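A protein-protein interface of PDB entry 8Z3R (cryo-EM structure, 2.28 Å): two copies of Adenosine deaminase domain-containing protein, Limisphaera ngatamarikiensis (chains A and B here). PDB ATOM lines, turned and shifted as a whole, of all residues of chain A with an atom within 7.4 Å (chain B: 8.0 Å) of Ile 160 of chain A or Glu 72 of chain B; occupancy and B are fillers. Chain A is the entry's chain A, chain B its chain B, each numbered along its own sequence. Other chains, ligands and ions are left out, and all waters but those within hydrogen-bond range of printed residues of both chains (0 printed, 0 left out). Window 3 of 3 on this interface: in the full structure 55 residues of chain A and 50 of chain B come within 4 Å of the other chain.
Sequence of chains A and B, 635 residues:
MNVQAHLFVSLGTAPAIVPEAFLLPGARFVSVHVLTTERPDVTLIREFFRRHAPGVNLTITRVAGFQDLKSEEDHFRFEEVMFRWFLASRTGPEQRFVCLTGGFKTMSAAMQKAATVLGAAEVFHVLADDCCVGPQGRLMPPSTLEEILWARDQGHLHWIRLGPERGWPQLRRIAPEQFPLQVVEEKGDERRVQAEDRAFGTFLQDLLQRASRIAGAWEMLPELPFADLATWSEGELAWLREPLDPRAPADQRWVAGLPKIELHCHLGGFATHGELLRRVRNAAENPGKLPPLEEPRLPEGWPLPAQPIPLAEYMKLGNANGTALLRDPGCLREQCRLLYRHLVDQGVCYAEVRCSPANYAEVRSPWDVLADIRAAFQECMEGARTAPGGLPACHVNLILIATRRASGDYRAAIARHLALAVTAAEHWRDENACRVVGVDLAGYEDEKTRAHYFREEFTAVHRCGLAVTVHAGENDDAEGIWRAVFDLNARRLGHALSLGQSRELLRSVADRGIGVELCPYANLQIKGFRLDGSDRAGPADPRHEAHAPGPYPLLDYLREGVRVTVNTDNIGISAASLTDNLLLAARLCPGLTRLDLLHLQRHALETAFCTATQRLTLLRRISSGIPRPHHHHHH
Of the printed residues of chain B, His 158 of chain A touches Lys 70 (3.6 Å).
Trp 159 of chain A touches none of the printed residues of chain B.
Of chain B, only Lys 70, Ser 71 and Glu 72 come within 4 Å of Ile 160 of chain A.
Printed residues of chain B within 4 Å of Leu 162 of chain A: His 75.
Of chain A, only Ile 160 (3.7 Å) and Arg 161 (3.6 Å) come within 4 Å of Glu 72 of chain B.
Printed residues of chain A within 4 Å of His 75 of chain B: Leu 162 (3.7 Å).
Glu 79 of chain B touches none of the printed residues of chain A.
Among the printed residues, pairs that only touch across the chains: His 125 of chain A with Thr 106 of chain B, Leu 127 of chain A with Leu 69 of chain B, His 158 of chain A with Lys 70 of chain B, Ile 160 of chain A with Lys 70 of chain B, Ile 160 of chain A with Ser 71 of chain B, Ile 160 of chain A with Glu 72 of chain B, Arg 161 of chain A with Glu 72 of chain B and Leu 162 of chain A with His 75 of chain B.
No position is printed for both chains.
Of the 8 pairs that touch across the chains among the printed residues, none has its exchanged pair printed and touching as well.
The backbone NH of Leu 162 of chain A sits at hydrogen-bond distance from the backbone carbonyl oxygen of Val 123 of chain A, 2.8 Å away.
The backbone carbonyl oxygen (O) of Ile 160 of chain A is in hydrogen-bond range of the backbone NH (N) of His 125 of chain A (2.6 Å).
OG of Ser 71 of chain B sits close to N of Glu 73 of chain B.
Hydrophobic or aromatic side chains of chain A within 4 Å of the printed part of chain B: His 125, Leu 127, His 158, Ile 160 and Leu 162.
Hydrophobic or aromatic side chains of chain B within 4 Å of the printed part of chain A: Leu 69 and His 75.
Among the printed residues, no Asp or Glu carboxylate lies within 4 Å of a Lys or Arg side-chain nitrogen of the other chain.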
ATOM      1  N   LEU A  24      -1.057  17.919 -29.999  1.00  0.00           N
ATOM      2  CA  LEU A  24       0.168  18.533 -30.487  1.00  0.00           C
ATOM      3  C   LEU A  24      -0.195  19.754 -31.318  1.00  0.00           C
ATOM      4  O   LEU A  24      -0.967  19.629 -32.282  1.00  0.00           O
ATOM      5  CB  LEU A  24       0.983  17.540 -31.315  1.00  0.00           C
ATOM      6  CG  LEU A  24       2.337  18.003 -31.855  1.00  0.00           C
ATOM      7  CD1 LEU A  24       3.284  18.334 -30.717  1.00  0.00           C
ATOM      8  CD2 LEU A  24       2.941  16.941 -32.751  1.00  0.00           C
ATOM      9  N   VAL A  98       5.964  10.066 -34.025  1.00  0.00           N
ATOM     10  CA  VAL A  98       6.365   9.139 -32.975  1.00  0.00           C
ATOM     11  C   VAL A  98       6.538   9.899 -31.668  1.00  0.00           C
ATOM     12  O   VAL A  98       7.193  10.946 -31.627  1.00  0.00           O
ATOM     13  CB  VAL A  98       7.659   8.391 -33.349  1.00  0.00           C
ATOM     14  CG1 VAL A  98       8.001   7.360 -32.289  1.00  0.00           C
ATOM     15  CG2 VAL A  98       7.511   7.729 -34.705  1.00  0.00           C
ATOM     16  N   GLU A 122       8.477  13.020 -37.468  1.00  0.00           N
ATOM     17  CA  GLU A 122       8.608  13.825 -36.260  1.00  0.00           C
ATOM     18  C   GLU A 122       8.714  12.939 -35.027  1.00  0.00           C
ATOM     19  O   GLU A 122       7.901  12.030 -34.836  1.00  0.00           O
ATOM     20  CB  GLU A 122       7.423  14.783 -36.121  1.00  0.00           C
ATOM     21  CG  GLU A 122       7.451  15.642 -34.866  1.00  0.00           C
ATOM     22  CD  GLU A 122       8.723  16.455 -34.740  1.00  0.00           C
ATOM     23  OE1 GLU A 122       9.702  15.949 -34.152  1.00  0.00           O
ATOM     24  OE2 GLU A 122       8.745  17.604 -35.227  1.00  0.00           O
ATOM     25  N   VAL A 123       9.714  13.194 -34.188  1.00  0.00           N
ATOM     26  CA  VAL A 123       9.897  12.490 -32.926  1.00  0.00           C
ATOM     27  C   VAL A 123       9.849  13.522 -31.810  1.00  0.00           C
ATOM     28  O   VAL A 123      10.610  14.496 -31.829  1.00  0.00           O
ATOM     29  CB  VAL A 123      11.223  11.711 -32.896  1.00  0.00           C
ATOM     30  CG1 VAL A 123      11.444  11.092 -31.528  1.00  0.00           C
ATOM     31  CG2 VAL A 123      11.238  10.648 -33.977  1.00  0.00           C
ATOM     32  N   PHE A 124       8.961  13.311 -30.840  1.00  0.00           N
ATOM     33  CA  PHE A 124       8.752  14.311 -29.805  1.00  0.00           C
ATOM     34  C   PHE A 124       8.470  13.642 -28.468  1.00  0.00           C
ATOM     35  O   PHE A 124       8.105  12.465 -28.397  1.00  0.00           O
ATOM     36  CB  PHE A 124       7.621  15.279 -30.184  1.00  0.00           C
ATOM     37  CG  PHE A 124       6.249  14.673 -30.128  1.00  0.00           C
ATOM     38  CD1 PHE A 124       5.784  13.885 -31.166  1.00  0.00           C
ATOM     39  CD2 PHE A 124       5.417  14.908 -29.049  1.00  0.00           C
ATOM     40  CE1 PHE A 124       4.521  13.333 -31.122  1.00  0.00           C
ATOM     41  CE2 PHE A 124       4.154  14.357 -29.000  1.00  0.00           C
ATOM     42  CZ  PHE A 124       3.706  13.570 -30.038  1.00  0.00           C
ATOM     43  N   HIS A 125       8.654  14.423 -27.404  1.00  0.00           N
ATOM     44  CA  HIS A 125       8.484  13.983 -26.025  1.00  0.00           C
ATOM     45  C   HIS A 125       7.667  15.034 -25.288  1.00  0.00           C
ATOM     46  O   HIS A 125       7.928  16.232 -25.426  1.00  0.00           O
ATOM     47  CB  HIS A 125       9.847  13.783 -25.350  1.00  0.00           C
ATOM     48  CG  HIS A 125       9.766  13.364 -23.916  1.00  0.00           C
ATOM     49  ND1 HIS A 125       9.036  12.273 -23.500  1.00  0.00           N
ATOM     50  CD2 HIS A 125      10.305  13.902 -22.797  1.00  0.00           C
ATOM     51  CE1 HIS A 125       9.138  12.150 -22.189  1.00  0.00           C
ATOM     52  NE2 HIS A 125       9.904  13.126 -21.738  1.00  0.00           N
ATOM     53  N   VAL A 126       6.683  14.590 -24.509  1.00  0.00           N
ATOM     54  CA  VAL A 126       5.721  15.481 -23.867  1.00  0.00           C
ATOM     55  C   VAL A 126       5.888  15.403 -22.355  1.00  0.00           C
ATOM     56  O   VAL A 126       6.057  14.316 -21.791  1.00  0.00           O
ATOM     57  CB  VAL A 126       4.277  15.142 -24.289  1.00  0.00           C
ATOM     58  CG1 VAL A 126       3.970  13.674 -24.042  1.00  0.00           C
ATOM     59  CG2 VAL A 126       3.278  16.034 -23.568  1.00  0.00           C
ATOM     60  N   LEU A 127       5.856  16.566 -21.703  1.00  0.00           N
ATOM     61  CA  LEU A 127       5.938  16.668 -20.253  1.00  0.00           C
ATOM     62  C   LEU A 127       4.798  17.532 -19.735  1.00  0.00           C
ATOM     63  O   LEU A 127       4.242  18.358 -20.462  1.00  0.00           O
ATOM     64  CB  LEU A 127       7.274  17.264 -19.796  1.00  0.00           C
ATOM     65  CG  LEU A 127       8.554  16.565 -20.244  1.00  0.00           C
ATOM     66  CD1 LEU A 127       9.674  17.573 -20.370  1.00  0.00           C
ATOM     67  CD2 LEU A 127       8.929  15.478 -19.257  1.00  0.00           C
ATOM     68  N   LEU A 157       1.968  22.453 -20.751  1.00  0.00           N
ATOM     69  CA  LEU A 157       2.504  21.368 -21.558  1.00  0.00           C
ATOM     70  C   LEU A 157       3.580  21.920 -22.483  1.00  0.00           C
ATOM     71  O   LEU A 157       3.533  23.087 -22.882  1.00  0.00           O
ATOM     72  CB  LEU A 157       1.399  20.681 -22.362  1.00  0.00           C
ATOM     73  CG  LEU A 157       0.230  20.187 -21.506  1.00  0.00           C
ATOM     74  CD1 LEU A 157      -1.035  20.007 -22.327  1.00  0.00           C
ATOM     75  CD2 LEU A 157       0.599  18.912 -20.788  1.00  0.00           C
ATOM     76  N   HIS A 158       4.553  21.080 -22.821  1.00  0.00           N
ATOM     77  CA  HIS A 158       5.776  21.576 -23.443  1.00  0.00           C
ATOM     78  C   HIS A 158       6.028  21.042 -24.845  1.00  0.00           C
ATOM     79  O   HIS A 158       6.349  21.828 -25.742  1.00  0.00           O
ATOM     80  CB  HIS A 158       6.968  21.253 -22.537  1.00  0.00           C
ATOM     81  CG  HIS A 158       6.965  22.028 -21.257  1.00  0.00           C
ATOM     82  ND1 HIS A 158       6.206  23.165 -21.082  1.00  0.00           N
ATOM     83  CD2 HIS A 158       7.615  21.826 -20.087  1.00  0.00           C
ATOM     84  CE1 HIS A 158       6.394  23.634 -19.861  1.00  0.00           C
ATOM     85  NE2 HIS A 158       7.244  22.840 -19.237  1.00  0.00           N
ATOM     86  N   TRP A 159       5.897  19.732 -25.064  1.00  0.00           N
ATOM     87  CA  TRP A 159       6.003  19.118 -26.391  1.00  0.00           C
ATOM     88  C   TRP A 159       7.370  19.395 -27.028  1.00  0.00           C
ATOM     89  O   TRP A 159       7.497  20.099 -28.032  1.00  0.00           O
ATOM     90  CB  TRP A 159       4.875  19.601 -27.311  1.00  0.00           C
ATOM     91  CG  TRP A 159       3.516  19.153 -26.895  1.00  0.00           C
ATOM     92  CD1 TRP A 159       3.043  17.876 -26.873  1.00  0.00           C
ATOM     93  CD2 TRP A 159       2.441  19.989 -26.456  1.00  0.00           C
ATOM     94  NE1 TRP A 159       1.741  17.864 -26.437  1.00  0.00           N
ATOM     95  CE2 TRP A 159       1.348  19.150 -26.175  1.00  0.00           C
ATOM     96  CE3 TRP A 159       2.300  21.366 -26.269  1.00  0.00           C
ATOM     97  CZ2 TRP A 159       0.131  19.641 -25.716  1.00  0.00           C
ATOM     98  CZ3 TRP A 159       1.090  21.852 -25.816  1.00  0.00           C
ATOM     99  CH2 TRP A 159       0.021  20.992 -25.547  1.00  0.00           C
ATOM    100  N   ILE A 160       8.399  18.823 -26.407  1.00  0.00           N
ATOM    101  CA  ILE A 160       9.748  18.897 -26.961  1.00  0.00           C
ATOM    102  C   ILE A 160       9.828  17.995 -28.185  1.00  0.00           C
ATOM    103  O   ILE A 160       9.662  16.775 -28.083  1.00  0.00           O
ATOM    104  CB  ILE A 160      10.800  18.502 -25.914  1.00  0.00           C
ATOM    105  CG1 ILE A 160      10.790  19.473 -24.730  1.00  0.00           C
ATOM    106  CG2 ILE A 160      12.180  18.438 -26.545  1.00  0.00           C
ATOM    107  CD1 ILE A 160       9.836  19.096 -23.624  1.00  0.00           C
ATOM    108  N   ARG A 161      10.093  18.591 -29.348  1.00  0.00           N
ATOM    109  CA  ARG A 161      10.120  17.872 -30.620  1.00  0.00           C
ATOM    110  C   ARG A 161      11.531  17.931 -31.201  1.00  0.00           C
ATOM    111  O   ARG A 161      12.038  19.011 -31.524  1.00  0.00           O
ATOM    112  CB  ARG A 161       9.064  18.439 -31.576  1.00  0.00           C
ATOM    113  CG  ARG A 161       9.307  19.860 -32.068  1.00  0.00           C
ATOM    114  CD  ARG A 161       8.160  20.375 -32.917  1.00  0.00           C
ATOM    115  NE  ARG A 161       6.947  20.581 -32.134  1.00  0.00           N
ATOM    116  CZ  ARG A 161       5.766  20.884 -32.654  1.00  0.00           C
ATOM    117  NH1 ARG A 161       5.594  20.991 -33.960  1.00  0.00           N
ATOM    118  NH2 ARG A 161       4.733  21.087 -31.842  1.00  0.00           N
ATOM    119  N   LEU A 162      12.182  16.772 -31.288  1.00  0.00           N
ATOM    120  CA  LEU A 162      13.572  16.690 -31.739  1.00  0.00           C
ATOM    121  C   LEU A 162      13.659  16.256 -33.207  1.00  0.00           C
ATOM    122  O   LEU A 162      14.170  15.198 -33.559  1.00  0.00           O
ATOM    123  CB  LEU A 162      14.365  15.789 -30.783  1.00  0.00           C
ATOM    124  CG  LEU A 162      14.112  14.300 -30.474  1.00  0.00           C
ATOM    125  CD1 LEU A 162      14.709  13.293 -31.452  1.00  0.00           C
ATOM    126  CD2 LEU A 162      14.570  13.988 -29.054  1.00  0.00           C
ATOM    127  N   GLY A 163      13.182  17.141 -34.080  1.00  0.00           N
ATOM    128  CA  GLY A 163      13.433  17.048 -35.503  1.00  0.00           C
ATOM    129  C   GLY A 163      12.885  15.821 -36.211  1.00  0.00           C
ATOM    130  O   GLY A 163      12.393  14.873 -35.590  1.00  0.00           O
ATOM    131  N   PHE B  66      21.845  23.345 -18.040  1.00  0.00           N
ATOM    132  CA  PHE B  66      20.691  22.462 -18.185  1.00  0.00           C
ATOM    133  C   PHE B  66      20.250  22.007 -16.801  1.00  0.00           C
ATOM    134  O   PHE B  66      20.924  21.185 -16.171  1.00  0.00           O
ATOM    135  CB  PHE B  66      21.024  21.271 -19.083  1.00  0.00           C
ATOM    136  CG  PHE B  66      19.871  20.341 -19.310  1.00  0.00           C
ATOM    137  CD1 PHE B  66      18.849  20.682 -20.171  1.00  0.00           C
ATOM    138  CD2 PHE B  66      19.823  19.114 -18.685  1.00  0.00           C
ATOM    139  CE1 PHE B  66      17.789  19.826 -20.389  1.00  0.00           C
ATOM    140  CE2 PHE B  66      18.767  18.251 -18.898  1.00  0.00           C
ATOM    141  CZ  PHE B  66      17.750  18.608 -19.752  1.00  0.00           C
ATOM    142  N   LEU B  69      14.167  20.937 -18.693  1.00  0.00           N
ATOM    143  CA  LEU B  69      13.931  21.060 -20.124  1.00  0.00           C
ATOM    144  C   LEU B  69      12.511  21.553 -20.368  1.00  0.00           C
ATOM    145  O   LEU B  69      11.556  21.042 -19.773  1.00  0.00           O
ATOM    146  CB  LEU B  69      14.164  19.734 -20.856  1.00  0.00           C
ATOM    147  CG  LEU B  69      13.173  18.574 -20.733  1.00  0.00           C
ATOM    148  CD1 LEU B  69      13.431  17.539 -21.821  1.00  0.00           C
ATOM    149  CD2 LEU B  69      13.192  17.934 -19.363  1.00  0.00           C
ATOM    150  N   LYS B  70      12.386  22.561 -21.217  1.00  0.00           N
ATOM    151  CA  LYS B  70      11.102  23.072 -21.674  1.00  0.00           C
ATOM    152  C   LYS B  70      10.996  23.111 -23.187  1.00  0.00           C
ATOM    153  O   LYS B  70       9.894  22.989 -23.729  1.00  0.00           O
ATOM    154  CB  LYS B  70      10.858  24.474 -21.098  1.00  0.00           C
ATOM    155  CG  LYS B  70      10.673  24.489 -19.590  1.00  0.00           C
ATOM    156  CD  LYS B  70      10.381  25.887 -19.074  1.00  0.00           C
ATOM    157  CE  LYS B  70      10.278  25.897 -17.559  1.00  0.00           C
ATOM    158  NZ  LYS B  70       9.081  25.147 -17.087  1.00  0.00           N
ATOM    159  N   SER B  71      12.115  23.277 -23.882  1.00  0.00           N
ATOM    160  CA  SER B  71      12.182  23.226 -25.334  1.00  0.00           C
ATOM    161  C   SER B  71      13.233  22.197 -25.746  1.00  0.00           C
ATOM    162  O   SER B  71      13.837  21.522 -24.909  1.00  0.00           O
ATOM    163  CB  SER B  71      12.488  24.611 -25.905  1.00  0.00           C
ATOM    164  OG  SER B  71      13.786  25.038 -25.532  1.00  0.00           O
ATOM    165  N   GLU B  72      13.446  22.078 -27.053  1.00  0.00           N
ATOM    166  CA  GLU B  72      14.434  21.155 -27.593  1.00  0.00           C
ATOM    167  C   GLU B  72      15.828  21.760 -27.670  1.00  0.00           C
ATOM    168  O   GLU B  72      16.773  21.054 -28.034  1.00  0.00           O
ATOM    169  CB  GLU B  72      14.010  20.670 -28.985  1.00  0.00           C
ATOM    170  CG  GLU B  72      13.807  21.773 -30.016  1.00  0.00           C
ATOM    171  CD  GLU B  72      12.470  22.477 -29.879  1.00  0.00           C
ATOM    172  OE1 GLU B  72      12.212  23.417 -30.659  1.00  0.00           O
ATOM    173  OE2 GLU B  72      11.674  22.085 -29.000  1.00  0.00           O
ATOM    174  N   GLU B  73      15.975  23.044 -27.338  1.00  0.00           N
ATOM    175  CA  GLU B  73      17.280  23.689 -27.427  1.00  0.00           C
ATOM    176  C   GLU B  73      18.281  23.058 -26.470  1.00  0.00           C
ATOM    177  O   GLU B  73      19.455  22.878 -26.815  1.00  0.00           O
ATOM    178  CB  GLU B  73      17.140  25.184 -27.147  1.00  0.00           C
ATOM    179  CG  GLU B  73      16.338  25.927 -28.198  1.00  0.00           C
ATOM    180  CD  GLU B  73      17.036  25.960 -29.546  1.00  0.00           C
ATOM    181  OE1 GLU B  73      18.285  25.977 -29.569  1.00  0.00           O
ATOM    182  OE2 GLU B  73      16.338  25.966 -30.582  1.00  0.00           O
ATOM    183  N   ASP B  74      17.838  22.723 -25.257  1.00  0.00           N
ATOM    184  CA  ASP B  74      18.759  22.222 -24.244  1.00  0.00           C
ATOM    185  C   ASP B  74      19.012  20.725 -24.389  1.00  0.00           C
ATOM    186  O   ASP B  74      20.026  20.212 -23.895  1.00  0.00           O
ATOM    187  CB  ASP B  74      18.221  22.551 -22.856  1.00  0.00           C
ATOM    188  CG  ASP B  74      16.768  22.164 -22.690  1.00  0.00           C
ATOM    189  OD1 ASP B  74      16.080  22.812 -21.877  1.00  0.00           O
ATOM    190  OD2 ASP B  74      16.317  21.209 -23.357  1.00  0.00           O
ATOM    191  N   HIS B  75      18.105  20.002 -25.046  1.00  0.00           N
ATOM    192  CA  HIS B  75      18.393  18.604 -25.341  1.00  0.00           C
ATOM    193  C   HIS B  75      19.583  18.490 -26.283  1.00  0.00           C
ATOM    194  O   HIS B  75      20.428  17.602 -26.120  1.00  0.00           O
ATOM    195  CB  HIS B  75      17.159  17.912 -25.922  1.00  0.00           C
ATOM    196  CG  HIS B  75      17.447  16.571 -26.521  1.00  0.00           C
ATOM    197  ND1 HIS B  75      17.441  15.410 -25.778  1.00  0.00           N
ATOM    198  CD2 HIS B  75      17.726  16.201 -27.793  1.00  0.00           C
ATOM    199  CE1 HIS B  75      17.723  14.386 -26.563  1.00  0.00           C
ATOM    200  NE2 HIS B  75      17.897  14.838 -27.791  1.00  0.00           N
ATOM    201  N   PHE B  76      19.680  19.395 -27.260  1.00  0.00           N
ATOM    202  CA  PHE B  76      20.822  19.388 -28.169  1.00  0.00           C
ATOM    203  C   PHE B  76      22.125  19.715 -27.446  1.00  0.00           C
ATOM    204  O   PHE B  76      23.161  19.093 -27.717  1.00  0.00           O
ATOM    205  CB  PHE B  76      20.591  20.369 -29.317  1.00  0.00           C
ATOM    206  CG  PHE B  76      19.345  20.094 -30.105  1.00  0.00           C
ATOM    207  CD1 PHE B  76      18.968  18.797 -30.401  1.00  0.00           C
ATOM    208  CD2 PHE B  76      18.555  21.135 -30.557  1.00  0.00           C
ATOM    209  CE1 PHE B  76      17.822  18.544 -31.127  1.00  0.00           C
ATOM    210  CE2 PHE B  76      17.408  20.889 -31.283  1.00  0.00           C
ATOM    211  CZ  PHE B  76      17.041  19.591 -31.568  1.00  0.00           C
ATOM    212  N   ARG B  77      22.108  20.702 -26.539  1.00  0.00           N
ATOM    213  CA  ARG B  77      23.328  21.006 -25.796  1.00  0.00           C
ATOM    214  C   ARG B  77      23.746  19.810 -24.952  1.00  0.00           C
ATOM    215  O   ARG B  77      24.936  19.469 -24.892  1.00  0.00           O
ATOM    216  CB  ARG B  77      23.168  22.258 -24.920  1.00  0.00           C
ATOM    217  CG  ARG B  77      22.218  22.126 -23.758  1.00  0.00           C
ATOM    218  CD  ARG B  77      22.084  23.386 -22.918  1.00  0.00           C
ATOM    219  NE  ARG B  77      21.492  24.509 -23.634  1.00  0.00           N
ATOM    220  CZ  ARG B  77      22.161  25.587 -24.022  1.00  0.00           C
ATOM    221  NH1 ARG B  77      23.455  25.718 -23.784  1.00  0.00           N
ATOM    222  NH2 ARG B  77      21.509  26.567 -24.641  1.00  0.00           N
ATOM    223  N   PHE B  78      22.778  19.141 -24.313  1.00  0.00           N
ATOM    224  CA  PHE B  78      23.110  17.937 -23.560  1.00  0.00           C
ATOM    225  C   PHE B  78      23.708  16.865 -24.461  1.00  0.00           C
ATOM    226  O   PHE B  78      24.682  16.207 -24.085  1.00  0.00           O
ATOM    227  CB  PHE B  78      21.880  17.386 -22.842  1.00  0.00           C
ATOM    228  CG  PHE B  78      22.059  15.976 -22.361  1.00  0.00           C
ATOM    229  CD1 PHE B  78      22.822  15.702 -21.241  1.00  0.00           C
ATOM    230  CD2 PHE B  78      21.482  14.919 -23.046  1.00  0.00           C
ATOM    231  CE1 PHE B  78      23.000  14.402 -20.807  1.00  0.00           C
ATOM    232  CE2 PHE B  78      21.658  13.621 -22.617  1.00  0.00           C
ATOM    233  CZ  PHE B  78      22.417  13.362 -21.495  1.00  0.00           C
ATOM    234  N   GLU B  79      23.130  16.662 -25.647  1.00  0.00           N
ATOM    235  CA  GLU B  79      23.628  15.622 -26.544  1.00  0.00           C
ATOM    236  C   GLU B  79      25.056  15.910 -26.994  1.00  0.00           C
ATOM    237  O   GLU B  79      25.902  15.005 -27.027  1.00  0.00           O
ATOM    238  CB  GLU B  79      22.702  15.484 -27.751  1.00  0.00           C
ATOM    239  CG  GLU B  79      23.083  14.371 -28.713  1.00  0.00           C
ATOM    240  CD  GLU B  79      22.106  14.241 -29.866  1.00  0.00           C
ATOM    241  OE1 GLU B  79      21.146  15.037 -29.921  1.00  0.00           O
ATOM    242  OE2 GLU B  79      22.298  13.345 -30.714  1.00  0.00           O
ATOM    243  N   THR B 106      14.470  11.253 -22.642  1.00  0.00           N
ATOM    244  CA  THR B 106      15.276  11.561 -23.815  1.00  0.00           C
ATOM    245  C   THR B 106      16.767  11.389 -23.567  1.00  0.00           C
ATOM    246  O   THR B 106      17.556  11.530 -24.506  1.00  0.00           O
ATOM    247  CB  THR B 106      14.998  12.991 -24.288  1.00  0.00           C
ATOM    248  OG1 THR B 106      15.104  13.895 -23.182  1.00  0.00           O
ATOM    249  CG2 THR B 106      13.604  13.090 -24.884  1.00  0.00           C
ATOM    250  N   ARG B 198      28.129  23.065 -32.347  1.00  0.00           N
ATOM    251  CA  ARG B 198      27.532  21.773 -32.663  1.00  0.00           C
ATOM    252  C   ARG B 198      28.277  21.082 -33.803  1.00  0.00           C
ATOM    253  O   ARG B 198      27.670  20.451 -34.669  1.00  0.00           O
ATOM    254  CB  ARG B 198      26.058  21.935 -33.023  1.00  0.00           C
ATOM    255  CG  ARG B 198      25.288  22.897 -32.127  1.00  0.00           C
ATOM    256  CD  ARG B 198      24.879  22.238 -30.824  1.00  0.00           C
ATOM    257  NE  ARG B 198      24.131  23.139 -29.955  1.00  0.00           N
ATOM    258  CZ  ARG B 198      22.869  23.494 -30.151  1.00  0.00           C
ATOM    259  NH1 ARG B 198      22.174  23.040 -31.182  1.00  0.00           N
ATOM    260  NH2 ARG B 198      22.286  24.322 -29.289  1.00  0.00           N
